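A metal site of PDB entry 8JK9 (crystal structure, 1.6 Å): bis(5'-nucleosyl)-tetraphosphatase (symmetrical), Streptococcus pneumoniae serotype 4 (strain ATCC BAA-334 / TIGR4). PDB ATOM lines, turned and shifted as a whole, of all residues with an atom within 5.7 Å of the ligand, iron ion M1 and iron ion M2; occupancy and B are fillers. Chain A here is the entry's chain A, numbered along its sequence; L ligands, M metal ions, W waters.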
ATOM      1  N   ARG A  26     -10.625 -18.678  -5.782  1.00  0.00           N
ATOM      2  CA  ARG A  26     -11.883 -17.950  -5.908  1.00  0.00           C
ATOM      3  C   ARG A  26     -12.056 -17.355  -7.312  1.00  0.00           C
ATOM      4  O   ARG A  26     -13.161 -17.408  -7.850  1.00  0.00           O
ATOM      5  CB  ARG A  26     -12.010 -16.860  -4.825  1.00  0.00           C
ATOM      6  CG  ARG A  26     -13.353 -16.115  -4.768  1.00  0.00           C
ATOM      7  CD  ARG A  26     -14.554 -17.027  -4.570  1.00  0.00           C
ATOM      8  NE  ARG A  26     -14.371 -17.920  -3.419  1.00  0.00           N
ATOM      9  CZ  ARG A  26     -15.253 -18.836  -3.022  1.00  0.00           C
ATOM     10  NH1 ARG A  26     -14.975 -19.586  -1.963  1.00  0.00           N
ATOM     11  NH2 ARG A  26     -16.399 -19.010  -3.666  1.00  0.00           N
ATOM     12  N   HIS A  29     -12.920 -20.175  -9.594  1.00  0.00           N
ATOM     13  CA  HIS A  29     -14.339 -20.449  -9.395  1.00  0.00           C
ATOM     14  C   HIS A  29     -15.205 -19.472 -10.196  1.00  0.00           C
ATOM     15  O   HIS A  29     -16.096 -19.908 -10.914  1.00  0.00           O
ATOM     16  CB  HIS A  29     -14.666 -20.439  -7.881  1.00  0.00           C
ATOM     17  CG  HIS A  29     -16.129 -20.306  -7.573  1.00  0.00           C
ATOM     18  ND1 HIS A  29     -17.028 -21.319  -7.819  1.00  0.00           N
ATOM     19  CD2 HIS A  29     -16.841 -19.293  -7.016  1.00  0.00           C
ATOM     20  CE1 HIS A  29     -18.237 -20.928  -7.446  1.00  0.00           C
ATOM     21  NE2 HIS A  29     -18.147 -19.710  -6.949  1.00  0.00           N
ATOM     22  N   VAL A  33     -17.959 -20.281 -13.068  1.00  0.00           N
ATOM     23  CA  VAL A  33     -19.357 -19.832 -13.052  1.00  0.00           C
ATOM     24  C   VAL A  33     -19.701 -19.046 -14.329  1.00  0.00           C
ATOM     25  O   VAL A  33     -20.781 -19.211 -14.881  1.00  0.00           O
ATOM     26  CB  VAL A  33     -19.672 -19.043 -11.749  1.00  0.00           C
ATOM     27  CG1 VAL A  33     -21.126 -18.570 -11.715  1.00  0.00           C
ATOM     28  CG2 VAL A  33     -19.411 -19.918 -10.546  1.00  0.00           C
ATOM     29  N   HIS A  58     -20.198 -12.769  -9.684  1.00  0.00           N
ATOM     30  CA  HIS A  58     -21.108 -13.088  -8.572  1.00  0.00           C
ATOM     31  C   HIS A  58     -20.399 -13.090  -7.202  1.00  0.00           C
ATOM     32  O   HIS A  58     -20.984 -12.630  -6.209  1.00  0.00           O
ATOM     33  CB  HIS A  58     -21.852 -14.406  -8.811  1.00  0.00           C
ATOM     34  CG  HIS A  58     -21.039 -15.608  -8.477  1.00  0.00           C
ATOM     35  ND1 HIS A  58     -20.002 -16.053  -9.263  1.00  0.00           N
ATOM     36  CD2 HIS A  58     -21.080 -16.427  -7.399  1.00  0.00           C
ATOM     37  CE1 HIS A  58     -19.445 -17.110  -8.695  1.00  0.00           C
ATOM     38  NE2 HIS A  58     -20.088 -17.356  -7.571  1.00  0.00           N
ATOM     39  N   ASP A  59     -19.138 -13.543  -7.162  1.00  0.00           N
ATOM     40  CA  ASP A  59     -18.356 -13.584  -5.925  1.00  0.00           C
ATOM     41  C   ASP A  59     -17.287 -12.483  -5.815  1.00  0.00           C
ATOM     42  O   ASP A  59     -16.339 -12.612  -5.023  1.00  0.00           O
ATOM     43  CB  ASP A  59     -17.706 -14.974  -5.714  1.00  0.00           C
ATOM     44  CG  ASP A  59     -18.643 -15.979  -5.052  1.00  0.00           C
ATOM     45  OD1 ASP A  59     -19.665 -15.592  -4.438  1.00  0.00           O
ATOM     46  OD2 ASP A  59     -18.346 -17.189  -5.173  1.00  0.00           O
ATOM     47  N   LYS A  62     -16.571 -11.408  -2.261  1.00  0.00           N
ATOM     48  CA  LYS A  62     -16.394 -12.509  -1.304  1.00  0.00           C
ATOM     49  C   LYS A  62     -15.436 -12.197  -0.148  1.00  0.00           C
ATOM     50  O   LYS A  62     -15.613 -12.705   0.970  1.00  0.00           O
ATOM     51  CB  LYS A  62     -15.935 -13.770  -2.038  1.00  0.00           C
ATOM     52  CG  LYS A  62     -15.845 -15.028  -1.196  1.00  0.00           C
ATOM     53  CD  LYS A  62     -17.202 -15.675  -0.954  1.00  0.00           C
ATOM     54  CE  LYS A  62     -17.058 -17.066  -0.375  1.00  0.00           C
ATOM     55  NZ  LYS A  62     -18.403 -17.673  -0.111  1.00  0.00           N
ATOM     56  N   TRP A  85     -26.123 -11.011  10.543  1.00  0.00           N
ATOM     57  CA  TRP A  85     -25.663 -12.138   9.724  1.00  0.00           C
ATOM     58  C   TRP A  85     -24.164 -11.984   9.434  1.00  0.00           C
ATOM     59  O   TRP A  85     -23.426 -11.450  10.275  1.00  0.00           O
ATOM     60  CB  TRP A  85     -26.568 -12.295   8.479  1.00  0.00           C
ATOM     61  CG  TRP A  85     -28.002 -12.560   8.890  1.00  0.00           C
ATOM     62  CD1 TRP A  85     -28.953 -11.616   9.163  1.00  0.00           C
ATOM     63  CD2 TRP A  85     -28.605 -13.826   9.152  1.00  0.00           C
ATOM     64  NE1 TRP A  85     -30.129 -12.216   9.543  1.00  0.00           N
ATOM     65  CE2 TRP A  85     -29.945 -13.571   9.555  1.00  0.00           C
ATOM     66  CE3 TRP A  85     -28.158 -15.148   9.064  1.00  0.00           C
ATOM     67  CZ2 TRP A  85     -30.833 -14.601   9.874  1.00  0.00           C
ATOM     68  CZ3 TRP A  85     -29.063 -16.175   9.378  1.00  0.00           C
ATOM     69  CH2 TRP A  85     -30.369 -15.890   9.785  1.00  0.00           C
ATOM     70  N   ASN A  88     -21.603 -14.914   4.362  1.00  0.00           N
ATOM     71  CA  ASN A  88     -22.469 -15.767   3.534  1.00  0.00           C
ATOM     72  C   ASN A  88     -23.662 -15.021   2.943  1.00  0.00           C
ATOM     73  O   ASN A  88     -23.898 -15.071   1.739  1.00  0.00           O
ATOM     74  CB  ASN A  88     -22.937 -17.008   4.304  1.00  0.00           C
ATOM     75  CG  ASN A  88     -21.810 -18.008   4.546  1.00  0.00           C
ATOM     76  OD1 ASN A  88     -20.696 -17.852   4.052  1.00  0.00           O
ATOM     77  ND2 ASN A  88     -22.117 -19.061   5.310  1.00  0.00           N
ATOM     78  N   VAL A  89     -24.378 -14.291   3.806  1.00  0.00           N
ATOM     79  CA  VAL A  89     -25.498 -13.457   3.369  1.00  0.00           C
ATOM     80  C   VAL A  89     -24.986 -12.185   2.675  1.00  0.00           C
ATOM     81  O   VAL A  89     -25.500 -11.807   1.627  1.00  0.00           O
ATOM     82  CB  VAL A  89     -26.434 -13.114   4.565  1.00  0.00           C
ATOM     83  CG1 VAL A  89     -27.525 -12.136   4.137  1.00  0.00           C
ATOM     84  CG2 VAL A  89     -27.075 -14.378   5.113  1.00  0.00           C
ATOM     85  N   HIS A  91     -22.135 -11.179   1.003  1.00  0.00           N
ATOM     86  CA  HIS A  91     -21.263 -10.992  -0.172  1.00  0.00           C
ATOM     87  C   HIS A  91     -22.055 -10.767  -1.455  1.00  0.00           C
ATOM     88  O   HIS A  91     -21.615 -10.011  -2.324  1.00  0.00           O
ATOM     89  CB  HIS A  91     -20.142 -12.034  -0.302  1.00  0.00           C
ATOM     90  CG  HIS A  91     -20.588 -13.392  -0.765  1.00  0.00           C
ATOM     91  ND1 HIS A  91     -21.264 -14.269   0.044  1.00  0.00           N
ATOM     92  CD2 HIS A  91     -20.425 -14.011  -1.956  1.00  0.00           C
ATOM     93  CE1 HIS A  91     -21.519 -15.383  -0.630  1.00  0.00           C
ATOM     94  NE2 HIS A  91     -21.019 -15.247  -1.844  1.00  0.00           N
ATOM     95  N   HIS A 117     -27.691 -14.563  -5.324  1.00  0.00           N
ATOM     96  CA  HIS A 117     -27.033 -15.799  -5.804  1.00  0.00           C
ATOM     97  C   HIS A 117     -26.822 -16.868  -4.714  1.00  0.00           C
ATOM     98  O   HIS A 117     -26.703 -18.049  -5.028  1.00  0.00           O
ATOM     99  CB  HIS A 117     -25.715 -15.518  -6.530  1.00  0.00           C
ATOM    100  CG  HIS A 117     -24.531 -15.380  -5.624  1.00  0.00           C
ATOM    101  ND1 HIS A 117     -24.092 -14.153  -5.160  1.00  0.00           N
ATOM    102  CD2 HIS A 117     -23.691 -16.303  -5.092  1.00  0.00           C
ATOM    103  CE1 HIS A 117     -23.037 -14.323  -4.383  1.00  0.00           C
ATOM    104  NE2 HIS A 117     -22.777 -15.625  -4.333  1.00  0.00           N
ATOM    105  N   THR A 118     -26.730 -16.430  -3.467  1.00  0.00           N
ATOM    106  CA  THR A 118     -26.481 -17.362  -2.359  1.00  0.00           C
ATOM    107  C   THR A 118     -27.793 -17.928  -1.798  1.00  0.00           C
ATOM    108  O   THR A 118     -27.927 -19.146  -1.613  1.00  0.00           O
ATOM    109  CB  THR A 118     -25.713 -16.685  -1.203  1.00  0.00           C
ATOM    110  OG1 THR A 118     -24.518 -16.066  -1.703  1.00  0.00           O
ATOM    111  CG2 THR A 118     -25.381 -17.663  -0.089  1.00  0.00           C
ATOM    112  N   VAL A 119     -28.747 -17.031  -1.540  1.00  0.00           N
ATOM    113  CA  VAL A 119     -29.968 -17.371  -0.822  1.00  0.00           C
ATOM    114  C   VAL A 119     -31.196 -17.595  -1.719  1.00  0.00           C
ATOM    115  O   VAL A 119     -32.172 -18.209  -1.287  1.00  0.00           O
ATOM    116  CB  VAL A 119     -30.276 -16.319   0.286  1.00  0.00           C
ATOM    117  CG1 VAL A 119     -29.142 -16.288   1.294  1.00  0.00           C
ATOM    118  CG2 VAL A 119     -30.514 -14.925  -0.299  1.00  0.00           C
ATOM    119  N   ASP A 135     -23.394 -21.375 -10.145  1.00  0.00           N
ATOM    120  CA  ASP A 135     -22.523 -21.299  -8.994  1.00  0.00           C
ATOM    121  C   ASP A 135     -22.271 -22.678  -8.363  1.00  0.00           C
ATOM    122  O   ASP A 135     -21.161 -23.005  -7.955  1.00  0.00           O
ATOM    123  CB  ASP A 135     -23.163 -20.351  -7.988  1.00  0.00           C
ATOM    124  CG  ASP A 135     -22.296 -20.085  -6.788  1.00  0.00           C
ATOM    125  OD1 ASP A 135     -21.053 -20.082  -6.908  1.00  0.00           O
ATOM    126  OD2 ASP A 135     -22.881 -19.851  -5.717  1.00  0.00           O
ATOM    127  N   ARG A 141     -16.162 -27.367  -8.968  1.00  0.00           N
ATOM    128  CA  ARG A 141     -16.848 -27.886  -7.785  1.00  0.00           C
ATOM    129  C   ARG A 141     -16.728 -29.389  -7.702  1.00  0.00           C
ATOM    130  O   ARG A 141     -16.897 -30.101  -8.702  1.00  0.00           O
ATOM    131  CB  ARG A 141     -18.331 -27.488  -7.749  1.00  0.00           C
ATOM    132  CG  ARG A 141     -18.628 -26.001  -7.616  1.00  0.00           C
ATOM    133  CD  ARG A 141     -18.530 -25.518  -6.172  1.00  0.00           C
ATOM    134  NE  ARG A 141     -19.387 -24.353  -5.949  1.00  0.00           N
ATOM    135  CZ  ARG A 141     -19.082 -23.310  -5.186  1.00  0.00           C
ATOM    136  NH1 ARG A 141     -19.952 -22.307  -5.064  1.00  0.00           N
ATOM    137  NH2 ARG A 141     -17.920 -23.244  -4.543  1.00  0.00           N
ATOM    138  N   GLU A 164     -30.730 -27.752  -5.369  1.00  0.00           N
ATOM    139  CA  GLU A 164     -29.700 -26.990  -4.659  1.00  0.00           C
ATOM    140  C   GLU A 164     -30.216 -26.414  -3.330  1.00  0.00           C
ATOM    141  O   GLU A 164     -29.543 -26.537  -2.287  1.00  0.00           O
ATOM    142  CB  GLU A 164     -29.127 -25.888  -5.547  1.00  0.00           C
ATOM    143  CG  GLU A 164     -28.144 -24.996  -4.794  1.00  0.00           C
ATOM    144  CD  GLU A 164     -27.537 -23.889  -5.632  1.00  0.00           C
ATOM    145  OE1 GLU A 164     -27.790 -23.843  -6.855  1.00  0.00           O
ATOM    146  OE2 GLU A 164     -26.805 -23.071  -5.039  1.00  0.00           O
ATOM    147  N   THR A 168     -28.965 -27.417   0.369  1.00  0.00           N
ATOM    148  CA  THR A 168     -28.380 -26.356   1.202  1.00  0.00           C
ATOM    149  C   THR A 168     -29.058 -26.248   2.569  1.00  0.00           C
ATOM    150  O   THR A 168     -28.371 -26.223   3.595  1.00  0.00           O
ATOM    151  CB  THR A 168     -28.367 -25.034   0.440  1.00  0.00           C
ATOM    152  OG1 THR A 168     -27.500 -25.213  -0.688  1.00  0.00           O
ATOM    153  CG2 THR A 168     -27.802 -23.907   1.315  1.00  0.00           C
ATOM    154  N   LEU A 172     -27.233 -27.029   6.080  1.00  0.00           N
ATOM    155  CA  LEU A 172     -27.159 -26.005   7.124  1.00  0.00           C
ATOM    156  C   LEU A 172     -27.678 -26.555   8.452  1.00  0.00           C
ATOM    157  O   LEU A 172     -27.034 -26.360   9.502  1.00  0.00           O
ATOM    158  CB  LEU A 172     -27.914 -24.740   6.702  1.00  0.00           C
ATOM    159  CG  LEU A 172     -27.275 -23.938   5.572  1.00  0.00           C
ATOM    160  CD1 LEU A 172     -28.313 -22.967   5.036  1.00  0.00           C
ATOM    161  CD2 LEU A 172     -25.998 -23.232   6.016  1.00  0.00           C
ATOM    162  N   PHE A 177     -26.051 -24.470  11.529  1.00  0.00           N
ATOM    163  CA  PHE A 177     -25.883 -23.057  11.192  1.00  0.00           C
ATOM    164  C   PHE A 177     -27.223 -22.359  10.994  1.00  0.00           C
ATOM    165  O   PHE A 177     -28.162 -22.980  10.487  1.00  0.00           O
ATOM    166  CB  PHE A 177     -25.074 -22.909   9.896  1.00  0.00           C
ATOM    167  CG  PHE A 177     -23.679 -23.505   9.947  1.00  0.00           C
ATOM    168  CD1 PHE A 177     -22.953 -23.552  11.142  1.00  0.00           C
ATOM    169  CD2 PHE A 177     -23.092 -23.984   8.782  1.00  0.00           C
ATOM    170  CE1 PHE A 177     -21.662 -24.090  11.162  1.00  0.00           C
ATOM    171  CE2 PHE A 177     -21.798 -24.508   8.798  1.00  0.00           C
ATOM    172  CZ  PHE A 177     -21.095 -24.568   9.982  1.00  0.00           C
ATOM    173  N   PRO A 178     -27.325 -21.069  11.372  1.00  0.00           N
ATOM    174  CA  PRO A 178     -28.583 -20.323  11.167  1.00  0.00           C
ATOM    175  C   PRO A 178     -28.972 -20.242   9.689  1.00  0.00           C
ATOM    176  O   PRO A 178     -28.096 -20.104   8.847  1.00  0.00           O
ATOM    177  CB  PRO A 178     -28.276 -18.912  11.699  1.00  0.00           C
ATOM    178  CG  PRO A 178     -26.985 -19.009  12.424  1.00  0.00           C
ATOM    179  CD  PRO A 178     -26.278 -20.258  12.025  1.00  0.00           C
ATOM    180  N   ILE A 179     -30.274 -20.327   9.409  1.00  0.00           N
ATOM    181  CA  ILE A 179     -30.776 -20.332   8.034  1.00  0.00           C
ATOM    182  C   ILE A 179     -31.439 -18.982   7.801  1.00  0.00           C
ATOM    183  O   ILE A 179     -32.390 -18.629   8.490  1.00  0.00           O
ATOM    184  CB  ILE A 179     -31.762 -21.501   7.803  1.00  0.00           C
ATOM    185  CG1 ILE A 179     -31.016 -22.829   7.923  1.00  0.00           C
ATOM    186  CG2 ILE A 179     -32.470 -21.384   6.449  1.00  0.00           C
ATOM    187  CD1 ILE A 179     -31.900 -24.035   8.158  1.00  0.00           C
ATOM    188  N   TYR A 180     -30.923 -18.253   6.819  1.00  0.00           N
ATOM    189  CA  TYR A 180     -31.475 -16.945   6.472  1.00  0.00           C
ATOM    190  C   TYR A 180     -32.937 -17.064   6.033  1.00  0.00           C
ATOM    191  O   TYR A 180     -33.267 -17.945   5.244  1.00  0.00           O
ATOM    192  CB  TYR A 180     -30.617 -16.286   5.372  1.00  0.00           C
ATOM    193  CG  TYR A 180     -30.906 -14.826   5.179  1.00  0.00           C
ATOM    194  CD1 TYR A 180     -30.725 -13.926   6.232  1.00  0.00           C
ATOM    195  CD2 TYR A 180     -31.316 -14.336   3.941  1.00  0.00           C
ATOM    196  CE1 TYR A 180     -30.984 -12.566   6.053  1.00  0.00           C
ATOM    197  CE2 TYR A 180     -31.578 -12.977   3.753  1.00  0.00           C
ATOM    198  CZ  TYR A 180     -31.406 -12.106   4.803  1.00  0.00           C
ATOM    199  OH  TYR A 180     -31.669 -10.768   4.586  1.00  0.00           O
ATOM    200  N   THR A 183     -33.642 -17.661   2.380  1.00  0.00           N
ATOM    201  CA  THR A 183     -33.328 -19.045   1.974  1.00  0.00           C
ATOM    202  C   THR A 183     -34.559 -19.956   2.086  1.00  0.00           C
ATOM    203  O   THR A 183     -34.841 -20.754   1.189  1.00  0.00           O
ATOM    204  CB  THR A 183     -32.141 -19.594   2.799  1.00  0.00           C
ATOM    205  OG1 THR A 183     -30.989 -18.785   2.527  1.00  0.00           O
ATOM    206  CG2 THR A 183     -31.820 -21.048   2.445  1.00  0.00           C
HETATM  207  P1  LIG L   1     -19.737 -19.493  -2.781  1.00  0.00           P
HETATM  208  O1  LIG L   1     -19.289 -19.871  -4.178  1.00  0.00           O
HETATM  209  O2  LIG L   1     -19.029 -20.317  -1.721  1.00  0.00           O
HETATM  210  O3  LIG L   1     -19.722 -18.000  -2.502  1.00  0.00           O
HETATM  211  O4  LIG L   1     -21.255 -20.047  -2.695  1.00  0.00           O
HETATM  212  P2  LIG L   1     -22.581 -19.336  -2.105  1.00  0.00           P
HETATM  213  O5  LIG L   1     -22.514 -17.837  -2.230  1.00  0.00           O
HETATM  214  O6  LIG L   1     -23.790 -20.039  -2.665  1.00  0.00           O
HETATM  215  O7  LIG L   1     -22.567 -19.734  -0.548  1.00  0.00           O
HETATM  216  C1  LIG L   1     -21.556 -19.407   0.378  1.00  0.00           C
HETATM  217  C2  LIG L   1     -21.865 -20.114   1.699  1.00  0.00           C
HETATM  218  O8  LIG L   1     -23.094 -19.558   2.186  1.00  0.00           O
HETATM  219  C3  LIG L   1     -22.055 -21.631   1.603  1.00  0.00           C
HETATM  220  O9  LIG L   1     -21.278 -22.284   2.631  1.00  0.00           O
HETATM  221  C4  LIG L   1     -23.544 -21.819   1.819  1.00  0.00           C
HETATM  222  O10 LIG L   1     -23.924 -23.073   2.391  1.00  0.00           O
HETATM  223  C5  LIG L   1     -23.845 -20.631   2.728  1.00  0.00           C
HETATM  224  N1  LIG L   1     -25.280 -20.331   2.890  1.00  0.00           N
HETATM  225  C6  LIG L   1     -26.236 -20.356   1.940  1.00  0.00           C
HETATM  226  N2  LIG L   1     -27.441 -20.046   2.476  1.00  0.00           N
HETATM  227  C7  LIG L   1     -27.232 -19.847   3.788  1.00  0.00           C
HETATM  228  C8  LIG L   1     -28.053 -19.492   4.947  1.00  0.00           C
HETATM  229  O11 LIG L   1     -29.269 -19.330   4.813  1.00  0.00           O
HETATM  230  N3  LIG L   1     -27.440 -19.396   6.144  1.00  0.00           N
HETATM  231  C9  LIG L   1     -26.111 -19.588   6.313  1.00  0.00           C
HETATM  232  N4  LIG L   1     -25.571 -19.468   7.547  1.00  0.00           N
HETATM  233  N5  LIG L   1     -25.283 -19.891   5.285  1.00  0.00           N
HETATM  234  C10 LIG L   1     -25.805 -20.023   4.046  1.00  0.00           C
HETATM  235 FE    FE M   1     -21.124 -16.666  -3.393  1.00  0.00          FE
HETATM  236 FE    FE M   2     -19.696 -18.701  -5.923  1.00  0.00          FE
HETATM  237 MG    MG M   3     -24.724 -13.587  -0.582  1.00  0.00          MG
HETATM  238  O   HOH W   1     -22.849 -22.550  -4.404  1.00  0.00           O
HETATM  239  O   HOH W   2     -29.121 -20.831   0.278  1.00  0.00           O
HETATM  240  O   HOH W   3     -20.063 -23.129  -1.356  1.00  0.00           O
HETATM  241  O   HOH W   4     -22.527 -22.605   5.731  1.00  0.00           O
HETATM  242  O   HOH W   5     -21.185 -17.953  -4.817  1.00  0.00           O
HETATM  243  O   HOH W   6     -25.492 -20.523  -5.020  1.00  0.00           O
HETATM  244  O   HOH W   7     -25.797 -21.119  -1.344  1.00  0.00           O
HETATM  245  O   HOH W   8     -17.788 -20.348   1.376  1.00  0.00           O
HETATM  246  O   HOH W   9     -16.927 -21.833  -2.119  1.00  0.00           O
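Water W5 bridges the side-chain carboxylate (OD2) of Asp 135 and an oxygen (O4) of the ligand. Water W9 lies within hydrogen-bond range of an oxygen (O2) of the ligand, the guanidinium group (NH2) of Arg 141 and the guanidinium group (NH1) of Arg 26. Water W7 bridges an oxygen (O6) of the ligand (2.6 Å) and the backbone carbonyl oxygen of Thr 118 (2.9 Å). Water W2 lies within hydrogen-bond range of O of Thr 118 (2.8 Å) and N2 of the ligand (2.9 Å). Water W1 lies within hydrogen-bond range of the guanidinium group of Arg 141, the side-chain carboxylate of Asp 135 and an oxygen (O6) of the ligand. Water W8 bridges NZ of Lys 62 and O2 of the ligand.
Iron ion M2 is bound by water W5 (2.0 Å). A ring nitrogen (NE2) of His 29 is bound to iron ion M2 (2.1 Å). O1 of the ligand binds iron ion M2 (2.1 Å). OD2 of Asp 59 binds iron ion M2. NE2 of His 58 binds iron ion M2 (2.2 Å). OD1 of Asp 135 is bound to iron ion M2 (2.2 Å). Iron ion M2 has six donor atoms within binding distance.
Iron ion M1 is bound by water W5 (1.9 Å), OD1 of Asp 59 (2.1 Å), NE2 of His 91 (2.1 Å), O3 of the ligand (2.1 Å), O5 of the ligand (2.2 Å) and NE2 of His 117 (2.2 Å).
Merely in contact with the ligand: Thr 168 (3.9 Å), Leu 172 (3.5 Å) and Ile 179 (3.7 Å). Hydrophobic or aromatic side chains that line the ligand: His 29, His 91, His 117, Leu 172 and Tyr 180. 16 residues have an atom within 4 Å of the ligand: Arg 26, His 29, Asp 59, Lys 62, Asn 88, His 91, His 117, Thr 118, Asp 135, Arg 141, Thr 168, Leu 172, Pro 178, Ile 179, Tyr 180 and Thr 183.
NH1 of Arg 141 is in salt-bridge range of O2 of the ligand (3.998 Å). An oxygen (O5) of the ligand lies close to the side-chain hydroxyl (OG1) of Thr 118 (2.7 Å). An oxygen (O2) of the ligand lies within salt-bridge range of the side-chain amino group (NZ) of Lys 62, 3.2 Å away. The backbone NH (N) of Tyr 180 sits at hydrogen-bond distance from an oxygen (O11) of the ligand (2.8 Å). N3 of the ligand is in hydrogen-bond range of O of Pro 178 (2.9 Å). O11 of the ligand is in hydrogen-bond range of OG1 of Thr 183, at 2.9 Å. NH2 of Arg 26 lies within salt-bridge range of O2 of the ligand. The side-chain amide nitrogen (ND2) of Asn 88 is in hydrogen-bond range of a nitrogen (N5) of the ligand (3.3 Å).
The side-chain carboxylate (OD2) of Asp 59 sits close to the guanidinium group (NH2) of Arg 26, 3.1 Å away. The backbone carbonyl oxygen (O) of Asn 88 lies within hydrogen-bond range of a ring nitrogen (ND1) of His 91 (3.2 Å). A ring nitrogen (NE2) of His 117 lies close to the side-chain hydroxyl of Thr 118 (3.2 Å). The guanidinium group of Arg 141 lies within salt-bridge range of the side-chain carboxylate of Asp 135 (3.9 Å). The backbone NH of Phe 177 lies within hydrogen-bond range of the backbone carbonyl oxygen of Leu 172 (2.9 Å). O of Glu 164 lies within hydrogen-bond range of OG1 of Thr 168 (2.9 Å).
Merely in contact with iron ion M2: Arg 141 (3.7 Å). Of the 23 residues printed, 5 come within 4 Å of iron ion M2. The nearest printed residue that does not touch iron ion M2 is Arg 26 (4.01 Å).
Residues that only touch iron ion M1: Thr 118 (3.8 Å). Four residues have an atom within 4 Å of iron ion M1: Asp 59, His 91, His 117 and Thr 118. The nearest printed residue that does not touch iron ion M1 is His 58 (4.01 Å).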
